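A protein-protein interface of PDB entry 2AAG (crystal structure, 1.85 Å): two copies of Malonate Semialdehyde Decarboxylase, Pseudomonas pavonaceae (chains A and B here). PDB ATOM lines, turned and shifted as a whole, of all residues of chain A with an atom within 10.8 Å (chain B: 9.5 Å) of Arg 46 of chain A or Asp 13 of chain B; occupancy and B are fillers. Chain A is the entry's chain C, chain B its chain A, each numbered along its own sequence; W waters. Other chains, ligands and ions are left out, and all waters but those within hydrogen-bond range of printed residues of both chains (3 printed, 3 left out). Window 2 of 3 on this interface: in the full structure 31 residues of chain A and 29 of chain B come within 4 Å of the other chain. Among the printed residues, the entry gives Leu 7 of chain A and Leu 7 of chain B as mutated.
A ring nitrogen (ND1) of His 45 of chain A sits at hydrogen-bond distance from the backbone carbonyl oxygen (O) of Val 42 of chain B (3.0 Å).
The side-chain amide nitrogen (NE2) of Gln 44 of chain B is in hydrogen-bond range of the side-chain carboxylate (OE2) of Glu 49 of chain A (2.7 Å).
The side-chain amide nitrogen (NE2) of Gln 44 of chain B sits close to the guanidinium group (NH1) of Arg 46 of chain A.
The backbone NH (N) of Val 42 of chain B sits at hydrogen-bond distance from the backbone carbonyl oxygen (O) of Glu 49 of chain A, 2.7 Å away.
OD2 of Asp 13 of chain B lies within salt-bridge range of NH2 of Arg 46 of chain A.
O of Val 51 of chain A lies within hydrogen-bond range of N of Gln 40 of chain B (2.9 Å).
Water W1 bridges the backbone carbonyl oxygen (O) of Asp 13 of chain B (2.6 Å) and the backbone carbonyl oxygen (O) of Gly 48 of chain A (3.2 Å).
Water W2 lies within hydrogen-bond range of the side-chain carboxylate of Asp 13 of chain B (2.7 Å), the backbone NH of Gly 48 of chain A (2.7 Å) and the guanidinium group of Arg 46 of chain A (2.7 Å).
Water W3 bridges OD1 of Asp 6 of chain A and OG of Ser 43 of chain B.
Arg 46 of chain A touches two residues of chain B.
Of chain A, only Arg 46 comes within 4 Å of Asp 13 of chain B.
No residue of chain B comes within 4 Å of Pro 47 of chain A.
Of chain B, only Ile 16 comes within 4 Å of Gly 48 of chain A.
Of chain B, only Thr 41, Val 42 and Gln 44 come within 4 Å of Glu 49 of chain A.
No residue of chain A comes within 4 Å of Ala 14 of chain B.
Ile 16 of chain B touches just one residue of chain A: Gly 48.
Printed residues of chain A within 4 Å of Thr 41 of chain B: Glu 49 and Met 50.
Printed residues of chain A within 4 Å of Gln 44 of chain B: Arg 46 and Glu 49.
Printed residues of chain A within 4 Å of Gln 40 of chain B: Met 50 and Val 51.
Gln 44 of chain A touches none of the printed residues of chain B.
The nearest residue of chain B that does not touch Arg 46 of chain A is Ile 16 of chain B (4.7 Å).
Among the printed residues, pairs that only touch across the chains: Met 50 of chain A with Gln 40 of chain B (3.2 Å), Glu 49 of chain A with Thr 41 of chain B (3.4 Å), Gly 48 of chain A with Ile 16 of chain B (3.5 Å) and Met 50 of chain A with Thr 41 of chain B (3.9 Å).
The backbone carbonyl oxygen (O) of His 45 of chain A is in hydrogen-bond range of the backbone NH (N) of Tyr 9 of chain A, 2.8 Å away.
O of Leu 20 of chain B lies within hydrogen-bond range of NE2 of Gln 40 of chain B, at 3.0 Å.
The side-chain carboxylate of Asp 6 of chain A lies within hydrogen-bond range of a ring nitrogen (NE2) of His 45 of chain A, 2.9 Å away.
Hydrophobic or aromatic side chains of chain A that line the printed part of chain B: His 45, Met 50 and Val 51.
Of the 19 printed residues of chain B, 6 touch a printed residue of chain A.
Hydrophobic or aromatic side chains of chain B that line the printed part of chain A: Ile 16 and Val 42.
Among the printed residues, Asp or Glu carboxylates within 4 Å of a Lys or Arg side-chain nitrogen of the other chain: Arg 46 of chain A with Asp 13 of chain B (2.6 Å).
Positions printed for both chains: 7, 9, 10, 11, 43 and 44.
Of the 10 pairs that touch across the chains among the printed residues, none has its exchanged pair printed and touching as well.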
ATOM      1  N   ASP A   6     -13.361  -2.184  -0.517  1.00  0.00           N
ATOM      2  CA  ASP A   6     -14.197  -3.345  -0.713  1.00  0.00           C
ATOM      3  C   ASP A   6     -14.928  -3.525   0.647  1.00  0.00           C
ATOM      4  O   ASP A   6     -14.296  -3.566   1.670  1.00  0.00           O
ATOM      5  CB  ASP A   6     -13.357  -4.586  -0.972  1.00  0.00           C
ATOM      6  CG  ASP A   6     -12.791  -4.630  -2.345  1.00  0.00           C
ATOM      7  OD1 ASP A   6     -13.585  -4.718  -3.283  1.00  0.00           O
ATOM      8  OD2 ASP A   6     -11.562  -4.633  -2.582  1.00  0.00           O
ATOM      9  N   LEU A   7     -16.244  -3.593   0.605  1.00  0.00           N
ATOM     10  CA  LEU A   7     -17.109  -3.731   1.790  1.00  0.00           C
ATOM     11  C   LEU A   7     -18.216  -4.710   1.444  1.00  0.00           C
ATOM     12  O   LEU A   7     -18.485  -5.026   0.241  1.00  0.00           O
ATOM     13  CB  LEU A   7     -17.697  -2.301   2.166  1.00  0.00           C
ATOM     14  CG  LEU A   7     -18.589  -1.667   1.088  1.00  0.00           C
ATOM     15  CD1 LEU A   7     -19.235  -0.281   1.497  1.00  0.00           C
ATOM     16  CD2 LEU A   7     -17.809  -1.398  -0.065  1.00  0.00           C
ATOM     17  N   PHE A   8     -18.892  -5.202   2.491  1.00  0.00           N
ATOM     18  CA  PHE A   8     -20.138  -5.937   2.314  1.00  0.00           C
ATOM     19  C   PHE A   8     -21.348  -5.008   2.117  1.00  0.00           C
ATOM     20  O   PHE A   8     -21.381  -3.840   2.637  1.00  0.00           O
ATOM     21  CB  PHE A   8     -20.418  -6.845   3.566  1.00  0.00           C
ATOM     22  CG  PHE A   8     -19.430  -8.005   3.683  1.00  0.00           C
ATOM     23  CD1 PHE A   8     -19.451  -9.037   2.724  1.00  0.00           C
ATOM     24  CD2 PHE A   8     -18.456  -8.038   4.687  1.00  0.00           C
ATOM     25  CE1 PHE A   8     -18.521 -10.105   2.766  1.00  0.00           C
ATOM     26  CE2 PHE A   8     -17.610  -9.171   4.806  1.00  0.00           C
ATOM     27  CZ  PHE A   8     -17.650 -10.177   3.815  1.00  0.00           C
ATOM     28  N   TYR A   9     -22.349  -5.526   1.389  1.00  0.00           N
ATOM     29  CA  TYR A   9     -23.624  -4.793   1.308  1.00  0.00           C
ATOM     30  C   TYR A   9     -24.205  -4.570   2.730  1.00  0.00           C
ATOM     31  O   TYR A   9     -23.987  -5.379   3.666  1.00  0.00           O
ATOM     32  CB  TYR A   9     -24.675  -5.569   0.468  1.00  0.00           C
ATOM     33  CG  TYR A   9     -24.543  -5.406  -1.023  1.00  0.00           C
ATOM     34  CD1 TYR A   9     -24.900  -4.222  -1.633  1.00  0.00           C
ATOM     35  CD2 TYR A   9     -24.076  -6.485  -1.846  1.00  0.00           C
ATOM     36  CE1 TYR A   9     -24.786  -4.054  -3.040  1.00  0.00           C
ATOM     37  CE2 TYR A   9     -23.973  -6.320  -3.276  1.00  0.00           C
ATOM     38  CZ  TYR A   9     -24.346  -5.112  -3.847  1.00  0.00           C
ATOM     39  OH  TYR A   9     -24.227  -4.832  -5.202  1.00  0.00           O
ATOM     40  N   GLY A  10     -24.888  -3.449   2.917  1.00  0.00           N
ATOM     41  CA  GLY A  10     -25.561  -3.205   4.168  1.00  0.00           C
ATOM     42  C   GLY A  10     -25.687  -1.735   4.543  1.00  0.00           C
ATOM     43  O   GLY A  10     -26.636  -1.296   5.229  1.00  0.00           O
ATOM     44  N   ARG A  11     -24.713  -0.952   4.141  1.00  0.00           N
ATOM     45  CA  ARG A  11     -24.755   0.473   4.485  1.00  0.00           C
ATOM     46  C   ARG A  11     -25.659   1.265   3.551  1.00  0.00           C
ATOM     47  O   ARG A  11     -25.820   0.907   2.356  1.00  0.00           O
ATOM     48  CB  ARG A  11     -23.355   1.059   4.336  1.00  0.00           C
ATOM     49  CG  ARG A  11     -22.369   0.622   5.385  1.00  0.00           C
ATOM     50  CD  ARG A  11     -21.003   1.053   4.998  1.00  0.00           C
ATOM     51  NE  ARG A  11     -19.954   0.833   6.015  1.00  0.00           N
ATOM     52  CZ  ARG A  11     -19.261  -0.298   6.192  1.00  0.00           C
ATOM     53  NH1 ARG A  11     -19.517  -1.412   5.466  1.00  0.00           N
ATOM     54  NH2 ARG A  11     -18.270  -0.321   7.084  1.00  0.00           N
ATOM     55  N   SER A  43     -16.620  -1.140  -3.923  1.00  0.00           N
ATOM     56  CA  SER A  43     -17.254  -2.357  -4.465  1.00  0.00           C
ATOM     57  C   SER A  43     -17.941  -2.996  -3.315  1.00  0.00           C
ATOM     58  O   SER A  43     -17.291  -3.156  -2.293  1.00  0.00           O
ATOM     59  CB  SER A  43     -16.212  -3.367  -4.993  1.00  0.00           C
ATOM     60  OG  SER A  43     -15.616  -2.728  -6.083  1.00  0.00           O
ATOM     61  N   GLN A  44     -19.243  -3.252  -3.464  1.00  0.00           N
ATOM     62  CA  GLN A  44     -20.018  -3.937  -2.429  1.00  0.00           C
ATOM     63  C   GLN A  44     -20.177  -5.400  -2.737  1.00  0.00           C
ATOM     64  O   GLN A  44     -20.359  -5.803  -3.911  1.00  0.00           O
ATOM     65  CB  GLN A  44     -21.374  -3.297  -2.247  1.00  0.00           C
ATOM     66  CG  GLN A  44     -21.268  -1.787  -1.891  1.00  0.00           C
ATOM     67  CD  GLN A  44     -22.568  -1.244  -1.346  1.00  0.00           C
ATOM     68  OE1 GLN A  44     -22.938  -1.585  -0.215  1.00  0.00           O
ATOM     69  NE2 GLN A  44     -23.249  -0.359  -2.117  1.00  0.00           N
ATOM     70  N   HIS A  45     -20.079  -6.218  -1.676  1.00  0.00           N
ATOM     71  CA  HIS A  45     -20.040  -7.646  -1.797  1.00  0.00           C
ATOM     72  C   HIS A  45     -21.145  -8.322  -0.971  1.00  0.00           C
ATOM     73  O   HIS A  45     -21.485  -7.930   0.150  1.00  0.00           O
ATOM     74  CB  HIS A  45     -18.668  -8.138  -1.303  1.00  0.00           C
ATOM     75  CG  HIS A  45     -17.520  -7.628  -2.123  1.00  0.00           C
ATOM     76  ND1 HIS A  45     -17.132  -8.191  -3.291  1.00  0.00           N
ATOM     77  CD2 HIS A  45     -16.680  -6.604  -1.956  1.00  0.00           C
ATOM     78  CE1 HIS A  45     -16.061  -7.564  -3.781  1.00  0.00           C
ATOM     79  NE2 HIS A  45     -15.802  -6.571  -3.011  1.00  0.00           N
ATOM     80  N   ARG A  46     -21.674  -9.406  -1.496  1.00  0.00           N
ATOM     81  CA  ARG A  46     -22.539 -10.311  -0.707  1.00  0.00           C
ATOM     82  C   ARG A  46     -21.676 -11.112   0.250  1.00  0.00           C
ATOM     83  O   ARG A  46     -20.477 -11.236   0.059  1.00  0.00           O
ATOM     84  CB  ARG A  46     -23.253 -11.245  -1.694  1.00  0.00           C
ATOM     85  CG  ARG A  46     -24.143 -10.454  -2.719  1.00  0.00           C
ATOM     86  CD  ARG A  46     -24.317 -11.216  -4.020  1.00  0.00           C
ATOM     87  NE  ARG A  46     -24.705 -12.520  -3.574  1.00  0.00           N
ATOM     88  CZ  ARG A  46     -23.990 -13.660  -3.641  1.00  0.00           C
ATOM     89  NH1 ARG A  46     -22.812 -13.796  -4.287  1.00  0.00           N
ATOM     90  NH2 ARG A  46     -24.527 -14.709  -3.035  1.00  0.00           N
ATOM     91  N   PRO A  47     -22.286 -11.676   1.294  1.00  0.00           N
ATOM     92  CA  PRO A  47     -21.551 -12.499   2.254  1.00  0.00           C
ATOM     93  C   PRO A  47     -20.663 -13.559   1.582  1.00  0.00           C
ATOM     94  O   PRO A  47     -19.569 -13.852   2.060  1.00  0.00           O
ATOM     95  CB  PRO A  47     -22.672 -13.211   3.002  1.00  0.00           C
ATOM     96  CG  PRO A  47     -23.791 -12.268   2.992  1.00  0.00           C
ATOM     97  CD  PRO A  47     -23.732 -11.589   1.618  1.00  0.00           C
ATOM     98  N   GLY A  48     -21.123 -14.146   0.489  1.00  0.00           N
ATOM     99  CA  GLY A  48     -20.212 -15.091  -0.172  1.00  0.00           C
ATOM    100  C   GLY A  48     -18.876 -14.571  -0.797  1.00  0.00           C
ATOM    101  O   GLY A  48     -18.062 -15.399  -1.308  1.00  0.00           O
ATOM    102  N   GLU A  49     -18.614 -13.262  -0.778  1.00  0.00           N
ATOM    103  CA  GLU A  49     -17.681 -12.740  -1.814  1.00  0.00           C
ATOM    104  C   GLU A  49     -16.471 -12.026  -1.243  1.00  0.00           C
ATOM    105  O   GLU A  49     -15.685 -11.467  -1.986  1.00  0.00           O
ATOM    106  CB  GLU A  49     -18.423 -11.798  -2.771  1.00  0.00           C
ATOM    107  CG  GLU A  49     -19.504 -12.482  -3.631  1.00  0.00           C
ATOM    108  CD  GLU A  49     -20.394 -11.468  -4.408  1.00  0.00           C
ATOM    109  OE1 GLU A  49     -20.432 -10.297  -3.975  1.00  0.00           O
ATOM    110  OE2 GLU A  49     -21.028 -11.803  -5.445  1.00  0.00           O
ATOM    111  N   MET A  50     -16.323 -12.006   0.088  1.00  0.00           N
ATOM    112  CA  MET A  50     -15.030 -11.666   0.693  1.00  0.00           C
ATOM    113  C   MET A  50     -14.804 -12.572   1.868  1.00  0.00           C
ATOM    114  O   MET A  50     -15.748 -12.904   2.611  1.00  0.00           O
ATOM    115  CB  MET A  50     -14.942 -10.196   1.220  1.00  0.00           C
ATOM    116  CG  MET A  50     -15.064  -9.079   0.213  1.00  0.00           C
ATOM    117  SD  MET A  50     -14.524  -7.557   1.060  1.00  0.00           S
ATOM    118  CE  MET A  50     -15.810  -7.315   2.376  1.00  0.00           C
ATOM    119  N   VAL A  51     -13.556 -12.970   2.045  1.00  0.00           N
ATOM    120  CA  VAL A  51     -13.116 -13.726   3.256  1.00  0.00           C
ATOM    121  C   VAL A  51     -11.899 -12.990   3.836  1.00  0.00           C
ATOM    122  O   VAL A  51     -10.860 -12.857   3.190  1.00  0.00           O
ATOM    123  CB  VAL A  51     -12.721 -15.151   2.881  1.00  0.00           C
ATOM    124  CG1 VAL A  51     -12.236 -15.887   4.100  1.00  0.00           C
ATOM    125  CG2 VAL A  51     -13.843 -15.831   2.318  1.00  0.00           C
ATOM    126  N   LEU A  52     -12.017 -12.512   5.071  1.00  0.00           N
ATOM    127  CA  LEU A  52     -10.948 -11.680   5.613  1.00  0.00           C
ATOM    128  C   LEU A  52     -10.671 -12.234   7.006  1.00  0.00           C
ATOM    129  O   LEU A  52     -11.517 -12.071   7.877  1.00  0.00           O
ATOM    130  CB  LEU A  52     -11.374 -10.198   5.651  1.00  0.00           C
ATOM    131  CG  LEU A  52     -11.652  -9.580   4.233  1.00  0.00           C
ATOM    132  CD1 LEU A  52     -12.485  -8.284   4.258  1.00  0.00           C
ATOM    133  CD2 LEU A  52     -10.420  -9.478   3.354  1.00  0.00           C
ATOM    134  N   SER A  62     -16.295  -7.959  11.673  1.00  0.00           N
ATOM    135  CA  SER A  62     -17.749  -8.022  11.534  1.00  0.00           C
ATOM    136  C   SER A  62     -18.161  -7.774  10.083  1.00  0.00           C
ATOM    137  O   SER A  62     -17.297  -7.628   9.246  1.00  0.00           O
ATOM    138  CB  SER A  62     -18.439  -6.978  12.397  1.00  0.00           C
ATOM    139  OG  SER A  62     -18.230  -5.652  11.847  1.00  0.00           O
ATOM    140  N   SER A  63     -19.475  -7.767   9.802  1.00  0.00           N
ATOM    141  CA  SER A  63     -19.938  -7.525   8.430  1.00  0.00           C
ATOM    142  C   SER A  63     -19.602  -6.064   8.050  1.00  0.00           C
ATOM    143  O   SER A  63     -19.651  -5.723   6.881  1.00  0.00           O
ATOM    144  CB  SER A  63     -21.431  -7.813   8.283  1.00  0.00           C
ATOM    145  OG  SER A  63     -22.126  -6.914   9.122  1.00  0.00           O
ATOM    146  N   VAL A  65     -16.642  -4.769   8.153  1.00  0.00           N
ATOM    147  CA  VAL A  65     -15.218  -4.749   7.779  1.00  0.00           C
ATOM    148  C   VAL A  65     -14.940  -4.009   6.447  1.00  0.00           C
ATOM    149  O   VAL A  65     -15.699  -4.167   5.452  1.00  0.00           O
ATOM    150  CB  VAL A  65     -14.652  -6.159   7.710  1.00  0.00           C
ATOM    151  CG1 VAL A  65     -15.067  -6.878   6.474  1.00  0.00           C
ATOM    152  CG2 VAL A  65     -13.244  -6.138   7.502  1.00  0.00           C
ATOM    153  N   LEU B   7     -14.577 -13.018 -11.822  1.00  0.00           N
ATOM    154  CA  LEU B   7     -15.236 -14.137 -12.506  1.00  0.00           C
ATOM    155  C   LEU B   7     -16.529 -13.643 -13.114  1.00  0.00           C
ATOM    156  O   LEU B   7     -17.000 -12.543 -12.756  1.00  0.00           O
ATOM    157  CB  LEU B   7     -15.548 -15.275 -11.505  1.00  0.00           C
ATOM    158  CG  LEU B   7     -16.551 -14.822 -10.406  1.00  0.00           C
ATOM    159  CD1 LEU B   7     -16.832 -15.941  -9.355  1.00  0.00           C
ATOM    160  CD2 LEU B   7     -15.917 -13.695  -9.683  1.00  0.00           C
ATOM    161  N   TYR B   9     -20.640 -13.997 -13.465  1.00  0.00           N
ATOM    162  CA  TYR B   9     -21.800 -14.554 -12.801  1.00  0.00           C
ATOM    163  C   TYR B   9     -22.133 -15.977 -13.233  1.00  0.00           C
ATOM    164  O   TYR B   9     -21.877 -16.390 -14.355  1.00  0.00           O
ATOM    165  CB  TYR B   9     -23.037 -13.645 -13.084  1.00  0.00           C
ATOM    166  CG  TYR B   9     -23.139 -12.425 -12.238  1.00  0.00           C
ATOM    167  CD1 TYR B   9     -23.522 -12.522 -10.885  1.00  0.00           C
ATOM    168  CD2 TYR B   9     -22.859 -11.171 -12.764  1.00  0.00           C
ATOM    169  CE1 TYR B   9     -23.628 -11.377 -10.098  1.00  0.00           C
ATOM    170  CE2 TYR B   9     -23.015 -10.007 -11.997  1.00  0.00           C
ATOM    171  CZ  TYR B   9     -23.400 -10.139 -10.664  1.00  0.00           C
ATOM    172  OH  TYR B   9     -23.456  -9.028  -9.858  1.00  0.00           O
ATOM    173  N   GLY B  10     -22.639 -16.782 -12.299  1.00  0.00           N
ATOM    174  CA  GLY B  10     -23.180 -18.075 -12.709  1.00  0.00           C
ATOM    175  C   GLY B  10     -22.927 -19.169 -11.705  1.00  0.00           C
ATOM    176  O   GLY B  10     -23.581 -20.195 -11.726  1.00  0.00           O
ATOM    177  N   ARG B  11     -21.978 -18.914 -10.805  1.00  0.00           N
ATOM    178  CA  ARG B  11     -21.663 -19.928  -9.775  1.00  0.00           C
ATOM    179  C   ARG B  11     -22.597 -19.736  -8.592  1.00  0.00           C
ATOM    180  O   ARG B  11     -23.061 -18.617  -8.315  1.00  0.00           O
ATOM    181  CB  ARG B  11     -20.212 -19.746  -9.271  1.00  0.00           C
ATOM    182  CG  ARG B  11     -19.122 -20.301 -10.262  1.00  0.00           C
ATOM    183  CD  ARG B  11     -17.788 -20.079  -9.703  1.00  0.00           C
ATOM    184  NE  ARG B  11     -16.663 -20.613 -10.515  1.00  0.00           N
ATOM    185  CZ  ARG B  11     -16.126 -20.015 -11.616  1.00  0.00           C
ATOM    186  NH1 ARG B  11     -16.628 -18.879 -12.116  1.00  0.00           N
ATOM    187  NH2 ARG B  11     -15.106 -20.587 -12.238  1.00  0.00           N
ATOM    188  N   THR B  12     -22.944 -20.850  -7.938  1.00  0.00           N
ATOM    189  CA  THR B  12     -23.542 -20.738  -6.619  1.00  0.00           C
ATOM    190  C   THR B  12     -22.538 -20.261  -5.597  1.00  0.00           C
ATOM    191  O   THR B  12     -21.319 -20.296  -5.792  1.00  0.00           O
ATOM    192  CB  THR B  12     -24.033 -22.122  -6.124  1.00  0.00           C
ATOM    193  OG1 THR B  12     -22.866 -22.967  -5.970  1.00  0.00           O
ATOM    194  CG2 THR B  12     -24.871 -22.870  -7.141  1.00  0.00           C
ATOM    195  N   ASP B  13     -23.014 -19.901  -4.418  1.00  0.00           N
ATOM    196  CA  ASP B  13     -22.145 -19.507  -3.374  1.00  0.00           C
ATOM    197  C   ASP B  13     -21.250 -20.663  -2.858  1.00  0.00           C
ATOM    198  O   ASP B  13     -20.116 -20.430  -2.461  1.00  0.00           O
ATOM    199  CB  ASP B  13     -22.941 -18.902  -2.278  1.00  0.00           C
ATOM    200  CG  ASP B  13     -23.168 -17.414  -2.495  1.00  0.00           C
ATOM    201  OD1 ASP B  13     -22.828 -16.842  -3.574  1.00  0.00           O
ATOM    202  OD2 ASP B  13     -23.636 -16.735  -1.603  1.00  0.00           O
ATOM    203  N   ALA B  14     -21.771 -21.889  -2.899  1.00  0.00           N
ATOM    204  CA  ALA B  14     -20.939 -23.066  -2.621  1.00  0.00           C
ATOM    205  C   ALA B  14     -19.733 -23.228  -3.579  1.00  0.00           C
ATOM    206  O   ALA B  14     -18.606 -23.482  -3.118  1.00  0.00           O
ATOM    207  CB  ALA B  14     -21.835 -24.340  -2.567  1.00  0.00           C
ATOM    208  N   GLN B  15     -19.941 -23.034  -4.887  1.00  0.00           N
ATOM    209  CA  GLN B  15     -18.894 -23.175  -5.889  1.00  0.00           C
ATOM    210  C   GLN B  15     -17.921 -22.003  -5.723  1.00  0.00           C
ATOM    211  O   GLN B  15     -16.744 -22.162  -5.933  1.00  0.00           O
ATOM    212  CB  GLN B  15     -19.507 -23.104  -7.303  1.00  0.00           C
ATOM    213  CG  GLN B  15     -20.363 -24.310  -7.627  1.00  0.00           C
ATOM    214  CD  GLN B  15     -21.127 -24.213  -8.961  1.00  0.00           C
ATOM    215  OE1 GLN B  15     -21.780 -23.177  -9.235  1.00  0.00           O
ATOM    216  NE2 GLN B  15     -21.073 -25.259  -9.755  1.00  0.00           N
ATOM    217  N   ILE B  16     -18.420 -20.818  -5.381  1.00  0.00           N
ATOM    218  CA  ILE B  16     -17.455 -19.741  -5.051  1.00  0.00           C
ATOM    219  C   ILE B  16     -16.570 -20.089  -3.825  1.00  0.00           C
ATOM    220  O   ILE B  16     -15.346 -19.836  -3.796  1.00  0.00           O
ATOM    221  CB  ILE B  16     -18.216 -18.416  -4.863  1.00  0.00           C
ATOM    222  CG1 ILE B  16     -18.668 -17.868  -6.228  1.00  0.00           C
ATOM    223  CG2 ILE B  16     -17.315 -17.384  -4.077  1.00  0.00           C
ATOM    224  CD1 ILE B  16     -19.632 -16.619  -6.189  1.00  0.00           C
ATOM    225  N   LYS B  17     -17.184 -20.640  -2.789  1.00  0.00           N
ATOM    226  CA  LYS B  17     -16.450 -21.035  -1.612  1.00  0.00           C
ATOM    227  C   LYS B  17     -15.435 -22.095  -1.903  1.00  0.00           C
ATOM    228  O   LYS B  17     -14.353 -22.031  -1.359  1.00  0.00           O
ATOM    229  CB  LYS B  17     -17.368 -21.471  -0.491  1.00  0.00           C
ATOM    230  CG  LYS B  17     -16.582 -21.812   0.824  1.00  0.00           C
ATOM    231  CD  LYS B  17     -17.529 -22.400   1.893  1.00  0.00           C
ATOM    232  CE  LYS B  17     -16.833 -22.516   3.257  1.00  0.00           C
ATOM    233  NZ  LYS B  17     -15.932 -23.636   3.348  1.00  0.00           N
ATOM    234  N   SER B  18     -15.774 -23.051  -2.765  1.00  0.00           N
ATOM    235  CA  SER B  18     -14.803 -24.084  -3.206  1.00  0.00           C
ATOM    236  C   SER B  18     -13.587 -23.490  -3.956  1.00  0.00           C
ATOM    237  O   SER B  18     -12.421 -23.884  -3.715  1.00  0.00           O
ATOM    238  CB  SER B  18     -15.482 -25.082  -4.171  1.00  0.00           C
ATOM    239  OG  SER B  18     -16.386 -25.912  -3.432  1.00  0.00           O
ATOM    240  N   LEU B  19     -13.871 -22.574  -4.873  1.00  0.00           N
ATOM    241  CA  LEU B  19     -12.814 -21.896  -5.618  1.00  0.00           C
ATOM    242  C   LEU B  19     -11.891 -21.107  -4.630  1.00  0.00           C
ATOM    243  O   LEU B  19     -10.675 -21.231  -4.710  1.00  0.00           O
ATOM    244  CB  LEU B  19     -13.503 -20.926  -6.546  1.00  0.00           C
ATOM    245  CG  LEU B  19     -12.814 -20.240  -7.711  1.00  0.00           C
ATOM    246  CD1 LEU B  19     -13.457 -18.878  -7.988  1.00  0.00           C
ATOM    247  CD2 LEU B  19     -11.269 -20.245  -7.741  1.00  0.00           C
ATOM    248  N   LEU B  20     -12.463 -20.313  -3.725  1.00  0.00           N
ATOM    249  CA  LEU B  20     -11.661 -19.561  -2.727  1.00  0.00           C
ATOM    250  C   LEU B  20     -10.835 -20.467  -1.803  1.00  0.00           C
ATOM    251  O   LEU B  20      -9.687 -20.165  -1.506  1.00  0.00           O
ATOM    252  CB  LEU B  20     -12.587 -18.720  -1.838  1.00  0.00           C
ATOM    253  CG  LEU B  20     -13.304 -17.597  -2.564  1.00  0.00           C
ATOM    254  CD1 LEU B  20     -14.159 -16.725  -1.609  1.00  0.00           C
ATOM    255  CD2 LEU B  20     -12.276 -16.731  -3.328  1.00  0.00           C
ATOM    256  N   ASP B  21     -11.448 -21.548  -1.325  1.00  0.00           N
ATOM    257  CA  ASP B  21     -10.702 -22.516  -0.444  1.00  0.00           C
ATOM    258  C   ASP B  21      -9.579 -23.191  -1.215  1.00  0.00           C
ATOM    259  O   ASP B  21      -8.452 -23.355  -0.694  1.00  0.00           O
ATOM    260  CB  ASP B  21     -11.674 -23.625   0.031  1.00  0.00           C
ATOM    261  CG  ASP B  21     -12.697 -23.138   1.035  1.00  0.00           C
ATOM    262  OD1 ASP B  21     -12.577 -22.000   1.540  1.00  0.00           O
ATOM    263  OD2 ASP B  21     -13.684 -23.832   1.421  1.00  0.00           O
ATOM    264  N   GLN B  40      -9.335 -12.365   0.755  1.00  0.00           N
ATOM    265  CA  GLN B  40      -9.772 -12.703  -0.571  1.00  0.00           C
ATOM    266  C   GLN B  40     -11.043 -11.873  -0.857  1.00  0.00           C
ATOM    267  O   GLN B  40     -11.869 -11.705   0.022  1.00  0.00           O
ATOM    268  CB  GLN B  40     -10.172 -14.180  -0.677  1.00  0.00           C
ATOM    269  CG  GLN B  40      -9.029 -15.129  -0.252  1.00  0.00           C
ATOM    270  CD  GLN B  40      -9.497 -16.570  -0.383  1.00  0.00           C
ATOM    271  OE1 GLN B  40     -10.575 -16.965   0.200  1.00  0.00           O
ATOM    272  NE2 GLN B  40      -8.772 -17.346  -1.195  1.00  0.00           N
ATOM    273  N   THR B  41     -11.180 -11.365  -2.093  1.00  0.00           N
ATOM    274  CA  THR B  41     -12.411 -10.718  -2.529  1.00  0.00           C
ATOM    275  C   THR B  41     -12.791 -11.342  -3.901  1.00  0.00           C
ATOM    276  O   THR B  41     -11.927 -11.866  -4.631  1.00  0.00           O
ATOM    277  CB  THR B  41     -12.240  -9.184  -2.740  1.00  0.00           C
ATOM    278  OG1 THR B  41     -11.270  -8.980  -3.786  1.00  0.00           O
ATOM    279  CG2 THR B  41     -11.614  -8.554  -1.534  1.00  0.00           C
ATOM    280  N   VAL B  42     -14.059 -11.312  -4.191  1.00  0.00           N
ATOM    281  CA  VAL B  42     -14.639 -11.870  -5.449  1.00  0.00           C
ATOM    282  C   VAL B  42     -15.478 -10.762  -6.100  1.00  0.00           C
ATOM    283  O   VAL B  42     -16.364 -10.198  -5.445  1.00  0.00           O
ATOM    284  CB  VAL B  42     -15.527 -13.090  -5.147  1.00  0.00           C
ATOM    285  CG1 VAL B  42     -16.121 -13.649  -6.486  1.00  0.00           C
ATOM    286  CG2 VAL B  42     -14.735 -14.133  -4.464  1.00  0.00           C
ATOM    287  N   SER B  43     -15.217 -10.466  -7.366  1.00  0.00           N
ATOM    288  CA  SER B  43     -16.075  -9.552  -8.143  1.00  0.00           C
ATOM    289  C   SER B  43     -16.724 -10.305  -9.298  1.00  0.00           C
ATOM    290  O   SER B  43     -16.025 -10.900 -10.126  1.00  0.00           O
ATOM    291  CB  SER B  43     -15.267  -8.354  -8.677  1.00  0.00           C
ATOM    292  OG  SER B  43     -14.718  -7.647  -7.565  1.00  0.00           O
ATOM    293  N   GLN B  44     -18.069 -10.304  -9.360  1.00  0.00           N
ATOM    294  CA  GLN B  44     -18.730 -11.042 -10.424  1.00  0.00           C
ATOM    295  C   GLN B  44     -19.116 -10.099 -11.554  1.00  0.00           C
ATOM    296  O   GLN B  44     -19.540  -8.979 -11.311  1.00  0.00           O
ATOM    297  CB  GLN B  44     -19.945 -11.809  -9.936  1.00  0.00           C
ATOM    298  CG  GLN B  44     -19.567 -12.761  -8.794  1.00  0.00           C
ATOM    299  CD  GLN B  44     -20.668 -13.790  -8.493  1.00  0.00           C
ATOM    300  OE1 GLN B  44     -20.980 -14.598  -9.326  1.00  0.00           O
ATOM    301  NE2 GLN B  44     -21.257 -13.709  -7.305  1.00  0.00           N
HETATM  302  O   HOH W   1     -19.351 -18.353  -1.071  1.00  0.00           O
HETATM  303  O   HOH W   2     -23.632 -14.309  -0.469  1.00  0.00           O
HETATM  304  O   HOH W   3     -13.162  -5.349  -6.069  1.00  0.00           O
